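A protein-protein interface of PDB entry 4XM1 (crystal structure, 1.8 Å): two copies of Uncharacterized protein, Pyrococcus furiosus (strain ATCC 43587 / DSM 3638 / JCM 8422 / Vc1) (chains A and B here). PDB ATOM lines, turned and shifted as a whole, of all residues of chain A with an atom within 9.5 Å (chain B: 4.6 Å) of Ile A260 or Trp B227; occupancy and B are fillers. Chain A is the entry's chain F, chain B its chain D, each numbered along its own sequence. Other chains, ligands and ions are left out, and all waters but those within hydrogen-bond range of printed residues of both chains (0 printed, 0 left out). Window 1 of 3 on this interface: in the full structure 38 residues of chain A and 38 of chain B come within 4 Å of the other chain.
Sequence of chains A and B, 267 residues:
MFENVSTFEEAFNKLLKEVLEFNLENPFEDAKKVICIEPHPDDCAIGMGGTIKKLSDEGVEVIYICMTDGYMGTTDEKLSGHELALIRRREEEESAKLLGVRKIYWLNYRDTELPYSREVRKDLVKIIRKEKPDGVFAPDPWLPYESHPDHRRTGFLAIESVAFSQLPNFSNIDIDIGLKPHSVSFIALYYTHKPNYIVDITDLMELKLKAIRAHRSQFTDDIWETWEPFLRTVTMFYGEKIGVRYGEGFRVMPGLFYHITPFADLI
Among the printed residues, pairs that only touch across the chains: Met A1 with Trp B224 (3.97 Å), Phe A2 with Pro B229 (3.4 Å), Val A19 with Thr B226 (3.8 Å), Leu A256 with Trp B227 (3.7 Å), Leu A256 with Phe B230 (3.4 Å), Tyr A258 with Glu B146 (3.9 Å), His A259 with His B151 (3.3 Å), Ile A260 with Leu B143 (3.6 Å), Ile A260 with His B151 (3.4 Å), Ile A260 with Tyr B191 (3.7 Å), Ile A260 with Trp B227 (3.8 Å), Ile A260 with Phe B230 (3.5 Å), Thr A261 with Leu B143 (3.9 Å), Thr A261 with Phe B230 (3.5 Å) and Pro A262 with Leu B143 (3.9 Å).
The backbone NH (N) of Ile A260 sits at hydrogen-bond distance from the side-chain carboxylate (OE1) of Glu B146 (2.8 Å).
The side-chain sulfur of Met A1 sits close to the side-chain carboxylate of Glu B225, at 3.5 Å.
The side-chain carboxylate of Glu B146 is in hydrogen-bond range of a ring nitrogen (ND1) of His A259, 2.6 Å away.
The side-chain carboxylate (OE1) of Glu B228 is in hydrogen-bond range of the backbone NH (N) of Met A1 (3.0 Å).
The backbone carbonyl oxygen (O) of Leu A256 is in hydrogen-bond range of the side-chain hydroxyl (OG1) of Thr A261 (3.1 Å).
The indole nitrogen (NE1) of Trp B224 is in hydrogen-bond range of the side-chain carboxylate (OE2) of Glu B228 (3.2 Å).
O of His A259 is in hydrogen-bond range of OG1 of Thr A261 (2.8 Å).
No position is printed for both chains.
Of chain B, only Leu B143 (3.6 Å), Glu B146 (2.8 Å), His B151 (3.4 Å), Tyr B191 (3.7 Å), Trp B227 (3.8 Å) and Phe B230 (3.5 Å) come within 4 Å of Ile A260.
Of chain A, only Leu A256 and Ile A260 come within 4 Å of Trp B227.
Printed residues of chain A within 4 Å of Glu B146: Tyr A258 (3.9 Å), His A259 (2.6 Å) and Ile A260 (2.8 Å).
Printed residues of chain A within 4 Å of His B151: His A259 and Ile A260.
Of the printed residues of chain B, Tyr A258 touches Glu B146 (3.9 Å).
Of the printed residues of chain B, Thr A261 touches Leu B143 (3.9 Å) and Phe B230 (3.5 Å).
Of the printed residues of chain A, Leu B143 touches Ile A260, Thr A261 and Pro A262.
Ile B223 touches none of the printed residues of chain A.
The nearest residue of chain B that does not touch Ile A260 is Ile B46 (4.2 Å).
The nearest residue of chain A that does not touch Trp B227 is His A259 (5.2 Å).
Hydrophobic or aromatic side chains of chain B that line the printed part of chain A: Leu B143, His B151, Tyr B191, Trp B224, Trp B227, Pro B229 and Phe B230.
Among the printed residues, no Asp or Glu carboxylate lies within 4 Å of a Lys or Arg side-chain nitrogen of the other chain.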
ATOM      1  N   MET A   1       8.499 -15.303  27.100  1.00  0.00           N
ATOM      2  CA  MET A   1       8.133 -16.308  26.076  1.00  0.00           C
ATOM      3  C   MET A   1       7.402 -15.634  24.925  1.00  0.00           C
ATOM      4  O   MET A   1       6.746 -14.624  25.129  1.00  0.00           O
ATOM      5  CB  MET A   1       7.240 -17.393  26.668  1.00  0.00           C
ATOM      6  CG  MET A   1       7.933 -18.125  27.709  1.00  0.00           C
ATOM      7  SD  MET A   1       7.074 -19.485  28.523  1.00  0.00           S
ATOM      8  CE  MET A   1       6.731 -18.634  30.059  1.00  0.00           C
ATOM      9  N   PHE A   2       7.491 -16.229  23.742  1.00  0.00           N
ATOM     10  CA  PHE A   2       6.746 -15.706  22.595  1.00  0.00           C
ATOM     11  C   PHE A   2       7.150 -14.287  22.275  1.00  0.00           C
ATOM     12  O   PHE A   2       6.346 -13.501  21.758  1.00  0.00           O
ATOM     13  CB  PHE A   2       5.224 -15.780  22.868  1.00  0.00           C
ATOM     14  CG  PHE A   2       4.579 -16.971  22.276  1.00  0.00           C
ATOM     15  CD1 PHE A   2       3.470 -16.847  21.449  1.00  0.00           C
ATOM     16  CD2 PHE A   2       5.137 -18.229  22.455  1.00  0.00           C
ATOM     17  CE1 PHE A   2       2.895 -17.980  20.887  1.00  0.00           C
ATOM     18  CE2 PHE A   2       4.586 -19.344  21.905  1.00  0.00           C
ATOM     19  CZ  PHE A   2       3.457 -19.244  21.117  1.00  0.00           C
ATOM     20  N   LEU A  15       1.236 -20.905  18.642  1.00  0.00           N
ATOM     21  CA  LEU A  15       0.336 -21.177  19.757  1.00  0.00           C
ATOM     22  C   LEU A  15      -0.419 -22.475  19.451  1.00  0.00           C
ATOM     23  O   LEU A  15      -0.458 -23.387  20.286  1.00  0.00           O
ATOM     24  CB  LEU A  15      -0.605 -19.974  19.976  1.00  0.00           C
ATOM     25  CG  LEU A  15      -1.681 -20.188  21.042  1.00  0.00           C
ATOM     26  CD1 LEU A  15      -1.048 -20.374  22.425  1.00  0.00           C
ATOM     27  CD2 LEU A  15      -2.675 -19.059  21.062  1.00  0.00           C
ATOM     28  N   VAL A  19       2.259 -24.841  21.486  1.00  0.00           N
ATOM     29  CA  VAL A  19       1.879 -24.664  22.897  1.00  0.00           C
ATOM     30  C   VAL A  19       0.686 -25.552  23.165  1.00  0.00           C
ATOM     31  O   VAL A  19       0.588 -26.186  24.224  1.00  0.00           O
ATOM     32  CB  VAL A  19       1.561 -23.183  23.244  1.00  0.00           C
ATOM     33  CG1 VAL A  19       1.164 -23.031  24.709  1.00  0.00           C
ATOM     34  CG2 VAL A  19       2.744 -22.263  22.913  1.00  0.00           C
ATOM     35  N   LEU A  20      -0.230 -25.606  22.206  1.00  0.00           N
ATOM     36  CA  LEU A  20      -1.484 -26.327  22.443  1.00  0.00           C
ATOM     37  C   LEU A  20      -1.491 -27.718  21.814  1.00  0.00           C
ATOM     38  O   LEU A  20      -2.355 -28.544  22.159  1.00  0.00           O
ATOM     39  CB  LEU A  20      -2.700 -25.508  21.977  1.00  0.00           C
ATOM     40  CG  LEU A  20      -2.857 -24.141  22.646  1.00  0.00           C
ATOM     41  CD1 LEU A  20      -3.926 -23.376  21.944  1.00  0.00           C
ATOM     42  CD2 LEU A  20      -3.224 -24.312  24.123  1.00  0.00           C
ATOM     43  N   MET A 253     -11.871 -27.899  18.877  1.00  0.00           N
ATOM     44  CA  MET A 253     -10.980 -26.811  19.273  1.00  0.00           C
ATOM     45  C   MET A 253     -10.132 -27.094  20.522  1.00  0.00           C
ATOM     46  O   MET A 253     -10.550 -27.851  21.352  1.00  0.00           O
ATOM     47  CB  MET A 253     -11.804 -25.506  19.512  1.00  0.00           C
ATOM     48  CG  MET A 253     -12.675 -25.044  18.337  1.00  0.00           C
ATOM     49  SD  MET A 253     -13.427 -23.393  18.601  1.00  0.00           S
ATOM     50  CE  MET A 253     -14.079 -23.580  20.264  1.00  0.00           C
ATOM     51  N   GLY A 255      -9.144 -26.586  24.244  1.00  0.00           N
ATOM     52  CA  GLY A 255     -10.020 -26.137  25.301  1.00  0.00           C
ATOM     53  C   GLY A 255      -9.878 -24.639  25.564  1.00  0.00           C
ATOM     54  O   GLY A 255     -10.874 -23.977  25.873  1.00  0.00           O
ATOM     55  N   LEU A 256      -8.674 -24.088  25.417  1.00  0.00           N
ATOM     56  CA  LEU A 256      -8.473 -22.621  25.575  1.00  0.00           C
ATOM     57  C   LEU A 256      -9.436 -21.725  24.756  1.00  0.00           C
ATOM     58  O   LEU A 256      -9.930 -20.679  25.257  1.00  0.00           O
ATOM     59  CB  LEU A 256      -7.000 -22.214  25.255  1.00  0.00           C
ATOM     60  CG  LEU A 256      -6.302 -21.042  25.907  1.00  0.00           C
ATOM     61  CD1 LEU A 256      -6.178 -21.214  27.447  1.00  0.00           C
ATOM     62  CD2 LEU A 256      -4.894 -20.941  25.273  1.00  0.00           C
ATOM     63  N   PHE A 257      -9.719 -22.171  23.534  1.00  0.00           N
ATOM     64  CA  PHE A 257     -10.469 -21.411  22.553  1.00  0.00           C
ATOM     65  C   PHE A 257     -11.935 -21.324  22.947  1.00  0.00           C
ATOM     66  O   PHE A 257     -12.689 -20.550  22.366  1.00  0.00           O
ATOM     67  CB  PHE A 257     -10.343 -22.048  21.183  1.00  0.00           C
ATOM     68  CG  PHE A 257      -9.072 -21.667  20.444  1.00  0.00           C
ATOM     69  CD1 PHE A 257      -7.865 -21.530  21.126  1.00  0.00           C
ATOM     70  CD2 PHE A 257      -9.103 -21.439  19.081  1.00  0.00           C
ATOM     71  CE1 PHE A 257      -6.708 -21.177  20.455  1.00  0.00           C
ATOM     72  CE2 PHE A 257      -7.965 -21.092  18.405  1.00  0.00           C
ATOM     73  CZ  PHE A 257      -6.770 -20.939  19.087  1.00  0.00           C
ATOM     74  N   TYR A 258     -12.368 -22.109  23.935  1.00  0.00           N
ATOM     75  CA  TYR A 258     -13.767 -21.988  24.419  1.00  0.00           C
ATOM     76  C   TYR A 258     -14.001 -20.790  25.395  1.00  0.00           C
ATOM     77  O   TYR A 258     -15.014 -20.726  26.115  1.00  0.00           O
ATOM     78  CB  TYR A 258     -14.258 -23.286  25.128  1.00  0.00           C
ATOM     79  CG  TYR A 258     -14.502 -24.428  24.157  1.00  0.00           C
ATOM     80  CD1 TYR A 258     -15.725 -24.547  23.481  1.00  0.00           C
ATOM     81  CD2 TYR A 258     -13.479 -25.367  23.881  1.00  0.00           C
ATOM     82  CE1 TYR A 258     -15.948 -25.584  22.590  1.00  0.00           C
ATOM     83  CE2 TYR A 258     -13.691 -26.438  22.973  1.00  0.00           C
ATOM     84  CZ  TYR A 258     -14.930 -26.538  22.349  1.00  0.00           C
ATOM     85  OH  TYR A 258     -15.225 -27.557  21.454  1.00  0.00           O
ATOM     86  N   HIS A 259     -13.038 -19.888  25.469  1.00  0.00           N
ATOM     87  CA  HIS A 259     -13.042 -18.869  26.517  1.00  0.00           C
ATOM     88  C   HIS A 259     -12.104 -17.754  26.091  1.00  0.00           C
ATOM     89  O   HIS A 259     -10.919 -18.013  25.729  1.00  0.00           O
ATOM     90  CB  HIS A 259     -12.593 -19.468  27.870  1.00  0.00           C
ATOM     91  CG  HIS A 259     -12.845 -18.573  29.066  1.00  0.00           C
ATOM     92  ND1 HIS A 259     -14.034 -17.908  29.277  1.00  0.00           N
ATOM     93  CD2 HIS A 259     -12.050 -18.250  30.119  1.00  0.00           C
ATOM     94  CE1 HIS A 259     -13.968 -17.218  30.394  1.00  0.00           C
ATOM     95  NE2 HIS A 259     -12.778 -17.421  30.942  1.00  0.00           N
ATOM     96  N   ILE A 260     -12.639 -16.540  26.143  1.00  0.00           N
ATOM     97  CA  ILE A 260     -11.904 -15.308  25.890  1.00  0.00           C
ATOM     98  C   ILE A 260     -10.890 -15.362  24.749  1.00  0.00           C
ATOM     99  O   ILE A 260      -9.812 -14.927  24.927  1.00  0.00           O
ATOM    100  CB  ILE A 260     -11.259 -14.680  27.140  1.00  0.00           C
ATOM    101  CG1 ILE A 260     -10.008 -15.472  27.602  1.00  0.00           C
ATOM    102  CG2 ILE A 260     -12.315 -14.428  28.167  1.00  0.00           C
ATOM    103  CD1 ILE A 260      -9.385 -14.967  28.914  1.00  0.00           C
ATOM    104  N   THR A 261     -11.262 -15.945  23.613  1.00  0.00           N
ATOM    105  CA  THR A 261     -10.349 -16.106  22.476  1.00  0.00           C
ATOM    106  C   THR A 261     -10.938 -15.399  21.254  1.00  0.00           C
ATOM    107  O   THR A 261     -11.766 -15.993  20.574  1.00  0.00           O
ATOM    108  CB  THR A 261     -10.142 -17.619  22.137  1.00  0.00           C
ATOM    109  OG1 THR A 261      -9.580 -18.267  23.289  1.00  0.00           O
ATOM    110  CG2 THR A 261      -9.125 -17.755  21.028  1.00  0.00           C
ATOM    111  N   PRO A 262     -10.486 -14.164  20.956  1.00  0.00           N
ATOM    112  CA  PRO A 262     -11.152 -13.466  19.817  1.00  0.00           C
ATOM    113  C   PRO A 262     -10.782 -13.961  18.415  1.00  0.00           C
ATOM    114  O   PRO A 262     -11.282 -13.434  17.356  1.00  0.00           O
ATOM    115  CB  PRO A 262     -10.730 -12.025  20.032  1.00  0.00           C
ATOM    116  CG  PRO A 262      -9.368 -12.144  20.611  1.00  0.00           C
ATOM    117  CD  PRO A 262      -9.342 -13.377  21.451  1.00  0.00           C
ATOM    118  N   PHE A 263      -9.919 -14.960  18.368  1.00  0.00           N
ATOM    119  CA  PHE A 263      -9.518 -15.592  17.118  1.00  0.00           C
ATOM    120  C   PHE A 263      -9.992 -17.072  17.033  1.00  0.00           C
ATOM    121  O   PHE A 263      -9.526 -17.869  16.182  1.00  0.00           O
ATOM    122  CB  PHE A 263      -7.989 -15.377  16.824  1.00  0.00           C
ATOM    123  CG  PHE A 263      -7.066 -15.725  17.986  1.00  0.00           C
ATOM    124  CD1 PHE A 263      -6.425 -14.720  18.692  1.00  0.00           C
ATOM    125  CD2 PHE A 263      -6.828 -17.073  18.335  1.00  0.00           C
ATOM    126  CE1 PHE A 263      -5.584 -15.043  19.801  1.00  0.00           C
ATOM    127  CE2 PHE A 263      -5.984 -17.414  19.428  1.00  0.00           C
ATOM    128  CZ  PHE A 263      -5.379 -16.403  20.164  1.00  0.00           C
ATOM    129  N   ALA A 264     -10.963 -17.410  17.881  1.00  0.00           N
ATOM    130  CA  ALA A 264     -11.585 -18.732  17.847  1.00  0.00           C
ATOM    131  C   ALA A 264     -12.098 -19.059  16.475  1.00  0.00           C
ATOM    132  O   ALA A 264     -11.910 -20.176  16.011  1.00  0.00           O
ATOM    133  CB  ALA A 264     -12.693 -18.898  18.904  1.00  0.00           C
ATOM    134  N   ILE B  46      -6.591  -8.929  32.827  1.00  0.00           N
ATOM    135  CA  ILE B  46      -6.398  -9.766  31.611  1.00  0.00           C
ATOM    136  C   ILE B  46      -6.962  -9.057  30.378  1.00  0.00           C
ATOM    137  O   ILE B  46      -6.247  -8.917  29.350  1.00  0.00           O
ATOM    138  CB  ILE B  46      -6.962 -11.205  31.826  1.00  0.00           C
ATOM    139  CG1 ILE B  46      -6.263 -11.876  33.042  1.00  0.00           C
ATOM    140  CG2 ILE B  46      -6.788 -12.106  30.664  1.00  0.00           C
ATOM    141  CD1 ILE B  46      -6.698 -13.310  33.244  1.00  0.00           C
ATOM    142  N   LEU B 143     -18.950 -12.471  22.214  1.00  0.00           N
ATOM    143  CA  LEU B 143     -17.683 -13.116  21.812  1.00  0.00           C
ATOM    144  C   LEU B 143     -17.925 -14.548  21.294  1.00  0.00           C
ATOM    145  O   LEU B 143     -18.525 -15.382  22.018  1.00  0.00           O
ATOM    146  CB  LEU B 143     -16.694 -13.145  22.994  1.00  0.00           C
ATOM    147  CG  LEU B 143     -15.325 -13.778  22.626  1.00  0.00           C
ATOM    148  CD1 LEU B 143     -14.611 -12.956  21.568  1.00  0.00           C
ATOM    149  CD2 LEU B 143     -14.501 -13.835  23.812  1.00  0.00           C
ATOM    150  N   GLU B 146     -17.572 -18.159  23.334  1.00  0.00           N
ATOM    151  CA  GLU B 146     -17.446 -17.977  24.790  1.00  0.00           C
ATOM    152  C   GLU B 146     -18.385 -18.933  25.490  1.00  0.00           C
ATOM    153  O   GLU B 146     -19.596 -18.872  25.316  1.00  0.00           O
ATOM    154  CB  GLU B 146     -17.810 -16.539  25.201  1.00  0.00           C
ATOM    155  CG  GLU B 146     -17.676 -16.219  26.680  1.00  0.00           C
ATOM    156  CD  GLU B 146     -16.357 -16.616  27.260  1.00  0.00           C
ATOM    157  OE1 GLU B 146     -15.309 -15.997  26.918  1.00  0.00           O
ATOM    158  OE2 GLU B 146     -16.384 -17.540  28.121  1.00  0.00           O
ATOM    159  N   HIS B 151     -19.193 -15.074  32.133  1.00  0.00           N
ATOM    160  CA  HIS B 151     -18.731 -14.052  31.183  1.00  0.00           C
ATOM    161  C   HIS B 151     -19.849 -13.463  30.312  1.00  0.00           C
ATOM    162  O   HIS B 151     -19.999 -12.254  30.287  1.00  0.00           O
ATOM    163  CB  HIS B 151     -17.548 -14.547  30.295  1.00  0.00           C
ATOM    164  CG  HIS B 151     -16.183 -14.422  30.942  1.00  0.00           C
ATOM    165  ND1 HIS B 151     -15.104 -13.915  30.256  1.00  0.00           N
ATOM    166  CD2 HIS B 151     -15.706 -14.756  32.179  1.00  0.00           C
ATOM    167  CE1 HIS B 151     -14.026 -13.962  31.015  1.00  0.00           C
ATOM    168  NE2 HIS B 151     -14.365 -14.409  32.205  1.00  0.00           N
ATOM    169  N   TYR B 191     -12.627  -8.059  25.596  1.00  0.00           N
ATOM    170  CA  TYR B 191     -12.678  -9.447  25.205  1.00  0.00           C
ATOM    171  C   TYR B 191     -13.558  -9.519  23.979  1.00  0.00           C
ATOM    172  O   TYR B 191     -14.617 -10.194  23.990  1.00  0.00           O
ATOM    173  CB  TYR B 191     -13.300 -10.287  26.319  1.00  0.00           C
ATOM    174  CG  TYR B 191     -12.449 -10.620  27.573  1.00  0.00           C
ATOM    175  CD1 TYR B 191     -11.088 -10.827  27.478  1.00  0.00           C
ATOM    176  CD2 TYR B 191     -13.064 -10.810  28.826  1.00  0.00           C
ATOM    177  CE1 TYR B 191     -10.303 -11.178  28.639  1.00  0.00           C
ATOM    178  CE2 TYR B 191     -12.319 -11.190  29.985  1.00  0.00           C
ATOM    179  CZ  TYR B 191     -10.915 -11.348  29.864  1.00  0.00           C
ATOM    180  OH  TYR B 191     -10.115 -11.716  30.932  1.00  0.00           O
ATOM    181  N   PHE B 219      -2.306 -18.321  38.259  1.00  0.00           N
ATOM    182  CA  PHE B 219      -1.193 -18.461  37.304  1.00  0.00           C
ATOM    183  C   PHE B 219       0.088 -19.031  37.959  1.00  0.00           C
ATOM    184  O   PHE B 219       1.004 -18.304  38.341  1.00  0.00           O
ATOM    185  CB  PHE B 219      -0.941 -17.179  36.517  1.00  0.00           C
ATOM    186  CG  PHE B 219      -2.156 -16.682  35.784  1.00  0.00           C
ATOM    187  CD1 PHE B 219      -2.486 -17.168  34.538  1.00  0.00           C
ATOM    188  CD2 PHE B 219      -2.995 -15.763  36.396  1.00  0.00           C
ATOM    189  CE1 PHE B 219      -3.628 -16.718  33.887  1.00  0.00           C
ATOM    190  CE2 PHE B 219      -4.169 -15.336  35.784  1.00  0.00           C
ATOM    191  CZ  PHE B 219      -4.478 -15.782  34.521  1.00  0.00           C
ATOM    192  N   ILE B 223       1.175 -23.233  34.412  1.00  0.00           N
ATOM    193  CA  ILE B 223       0.049 -22.612  33.782  1.00  0.00           C
ATOM    194  C   ILE B 223       0.557 -21.468  32.937  1.00  0.00           C
ATOM    195  O   ILE B 223       0.132 -21.339  31.788  1.00  0.00           O
ATOM    196  CB  ILE B 223      -1.077 -22.133  34.795  1.00  0.00           C
ATOM    197  CG1 ILE B 223      -1.854 -23.350  35.328  1.00  0.00           C
ATOM    198  CG2 ILE B 223      -2.015 -21.182  34.087  1.00  0.00           C
ATOM    199  CD1 ILE B 223      -2.533 -23.143  36.698  1.00  0.00           C
ATOM    200  N   TRP B 224       1.464 -20.660  33.487  1.00  0.00           N
ATOM    201  CA  TRP B 224       2.068 -19.551  32.734  1.00  0.00           C
ATOM    202  C   TRP B 224       2.762 -19.920  31.404  1.00  0.00           C
ATOM    203  O   TRP B 224       2.745 -19.116  30.446  1.00  0.00           O
ATOM    204  CB  TRP B 224       2.988 -18.748  33.636  1.00  0.00           C
ATOM    205  CG  TRP B 224       3.219 -17.336  33.140  1.00  0.00           C
ATOM    206  CD1 TRP B 224       4.397 -16.825  32.705  1.00  0.00           C
ATOM    207  CD2 TRP B 224       2.254 -16.254  33.044  1.00  0.00           C
ATOM    208  NE1 TRP B 224       4.239 -15.516  32.340  1.00  0.00           N
ATOM    209  CE2 TRP B 224       2.940 -15.138  32.543  1.00  0.00           C
ATOM    210  CE3 TRP B 224       0.880 -16.128  33.336  1.00  0.00           C
ATOM    211  CZ2 TRP B 224       2.302 -13.905  32.292  1.00  0.00           C
ATOM    212  CZ3 TRP B 224       0.254 -14.902  33.112  1.00  0.00           C
ATOM    213  CH2 TRP B 224       0.966 -13.806  32.595  1.00  0.00           C
ATOM    214  N   GLU B 225       3.375 -21.117  31.343  1.00  0.00           N
ATOM    215  CA  GLU B 225       3.915 -21.655  30.045  1.00  0.00           C
ATOM    216  C   GLU B 225       2.938 -21.579  28.909  1.00  0.00           C
ATOM    217  O   GLU B 225       3.330 -21.304  27.739  1.00  0.00           O
ATOM    218  CB  GLU B 225       4.393 -23.093  30.191  1.00  0.00           C
ATOM    219  CG  GLU B 225       5.555 -23.252  31.229  1.00  0.00           C
ATOM    220  CD  GLU B 225       6.791 -22.415  30.857  1.00  0.00           C
ATOM    221  OE1 GLU B 225       7.094 -21.337  31.450  1.00  0.00           O
ATOM    222  OE2 GLU B 225       7.549 -22.827  29.916  1.00  0.00           O
ATOM    223  N   THR B 226       1.656 -21.803  29.227  1.00  0.00           N
ATOM    224  CA  THR B 226       0.586 -21.681  28.202  1.00  0.00           C
ATOM    225  C   THR B 226       0.027 -20.255  28.036  1.00  0.00           C
ATOM    226  O   THR B 226      -0.209 -19.766  26.898  1.00  0.00           O
ATOM    227  CB  THR B 226      -0.543 -22.711  28.456  1.00  0.00           C
ATOM    228  OG1 THR B 226       0.007 -24.040  28.340  1.00  0.00           O
ATOM    229  CG2 THR B 226      -1.663 -22.571  27.469  1.00  0.00           C
ATOM    230  N   TRP B 227      -0.193 -19.601  29.165  1.00  0.00           N
ATOM    231  CA  TRP B 227      -0.887 -18.296  29.200  1.00  0.00           C
ATOM    232  C   TRP B 227      -0.056 -17.111  28.739  1.00  0.00           C
ATOM    233  O   TRP B 227      -0.575 -16.207  28.049  1.00  0.00           O
ATOM    234  CB  TRP B 227      -1.503 -18.079  30.584  1.00  0.00           C
ATOM    235  CG  TRP B 227      -2.807 -18.720  30.591  1.00  0.00           C
ATOM    236  CD1 TRP B 227      -3.050 -20.080  30.658  1.00  0.00           C
ATOM    237  CD2 TRP B 227      -4.087 -18.091  30.411  1.00  0.00           C
ATOM    238  NE1 TRP B 227      -4.394 -20.320  30.564  1.00  0.00           N
ATOM    239  CE2 TRP B 227      -5.059 -19.125  30.411  1.00  0.00           C
ATOM    240  CE3 TRP B 227      -4.508 -16.761  30.242  1.00  0.00           C
ATOM    241  CZ2 TRP B 227      -6.445 -18.875  30.264  1.00  0.00           C
ATOM    242  CZ3 TRP B 227      -5.905 -16.505  30.104  1.00  0.00           C
ATOM    243  CH2 TRP B 227      -6.846 -17.567  30.121  1.00  0.00           C
ATOM    244  N   GLU B 228       1.246 -17.087  29.075  1.00  0.00           N
ATOM    245  CA  GLU B 228       2.062 -15.999  28.542  1.00  0.00           C
ATOM    246  C   GLU B 228       1.996 -16.049  27.026  1.00  0.00           C
ATOM    247  O   GLU B 228       1.638 -15.083  26.398  1.00  0.00           O
ATOM    248  CB  GLU B 228       3.509 -15.909  29.077  1.00  0.00           C
ATOM    249  CG  GLU B 228       4.200 -14.697  28.452  1.00  0.00           C
ATOM    250  CD  GLU B 228       5.656 -14.475  28.860  1.00  0.00           C
ATOM    251  OE1 GLU B 228       6.248 -13.610  28.230  1.00  0.00           O
ATOM    252  OE2 GLU B 228       6.190 -15.140  29.774  1.00  0.00           O
ATOM    253  N   PRO B 229       2.222 -17.210  26.415  1.00  0.00           N
ATOM    254  CA  PRO B 229       2.065 -17.107  24.956  1.00  0.00           C
ATOM    255  C   PRO B 229       0.658 -16.728  24.465  1.00  0.00           C
ATOM    256  O   PRO B 229       0.541 -16.038  23.436  1.00  0.00           O
ATOM    257  CB  PRO B 229       2.400 -18.510  24.472  1.00  0.00           C
ATOM    258  CG  PRO B 229       3.327 -19.061  25.557  1.00  0.00           C
ATOM    259  CD  PRO B 229       2.775 -18.511  26.822  1.00  0.00           C
ATOM    260  N   PHE B 230      -0.370 -17.251  25.129  1.00  0.00           N
ATOM    261  CA  PHE B 230      -1.768 -16.922  24.809  1.00  0.00           C
ATOM    262  C   PHE B 230      -2.005 -15.403  24.861  1.00  0.00           C
ATOM    263  O   PHE B 230      -2.424 -14.793  23.857  1.00  0.00           O
ATOM    264  CB  PHE B 230      -2.713 -17.668  25.778  1.00  0.00           C
ATOM    265  CG  PHE B 230      -4.169 -17.372  25.551  1.00  0.00           C
ATOM    266  CD1 PHE B 230      -4.777 -17.709  24.358  1.00  0.00           C
ATOM    267  CD2 PHE B 230      -4.955 -16.800  26.548  1.00  0.00           C
ATOM    268  CE1 PHE B 230      -6.164 -17.473  24.176  1.00  0.00           C
ATOM    269  CE2 PHE B 230      -6.340 -16.554  26.341  1.00  0.00           C
ATOM    270  CZ  PHE B 230      -6.915 -16.873  25.154  1.00  0.00           C
ATOM    271  N   LEU B 231      -1.665 -14.795  25.991  1.00  0.00           N
ATOM    272  CA  LEU B 231      -1.820 -13.369  26.197  1.00  0.00           C
ATOM    273  C   LEU B 231      -1.072 -12.524  25.141  1.00  0.00           C
ATOM    274  O   LEU B 231      -1.623 -11.528  24.663  1.00  0.00           O
ATOM    275  CB  LEU B 231      -1.379 -12.979  27.607  1.00  0.00           C
ATOM    276  CG  LEU B 231      -2.275 -13.550  28.728  1.00  0.00           C
ATOM    277  CD1 LEU B 231      -1.567 -13.545  30.114  1.00  0.00           C
ATOM    278  CD2 LEU B 231      -3.635 -12.853  28.792  1.00  0.00           C
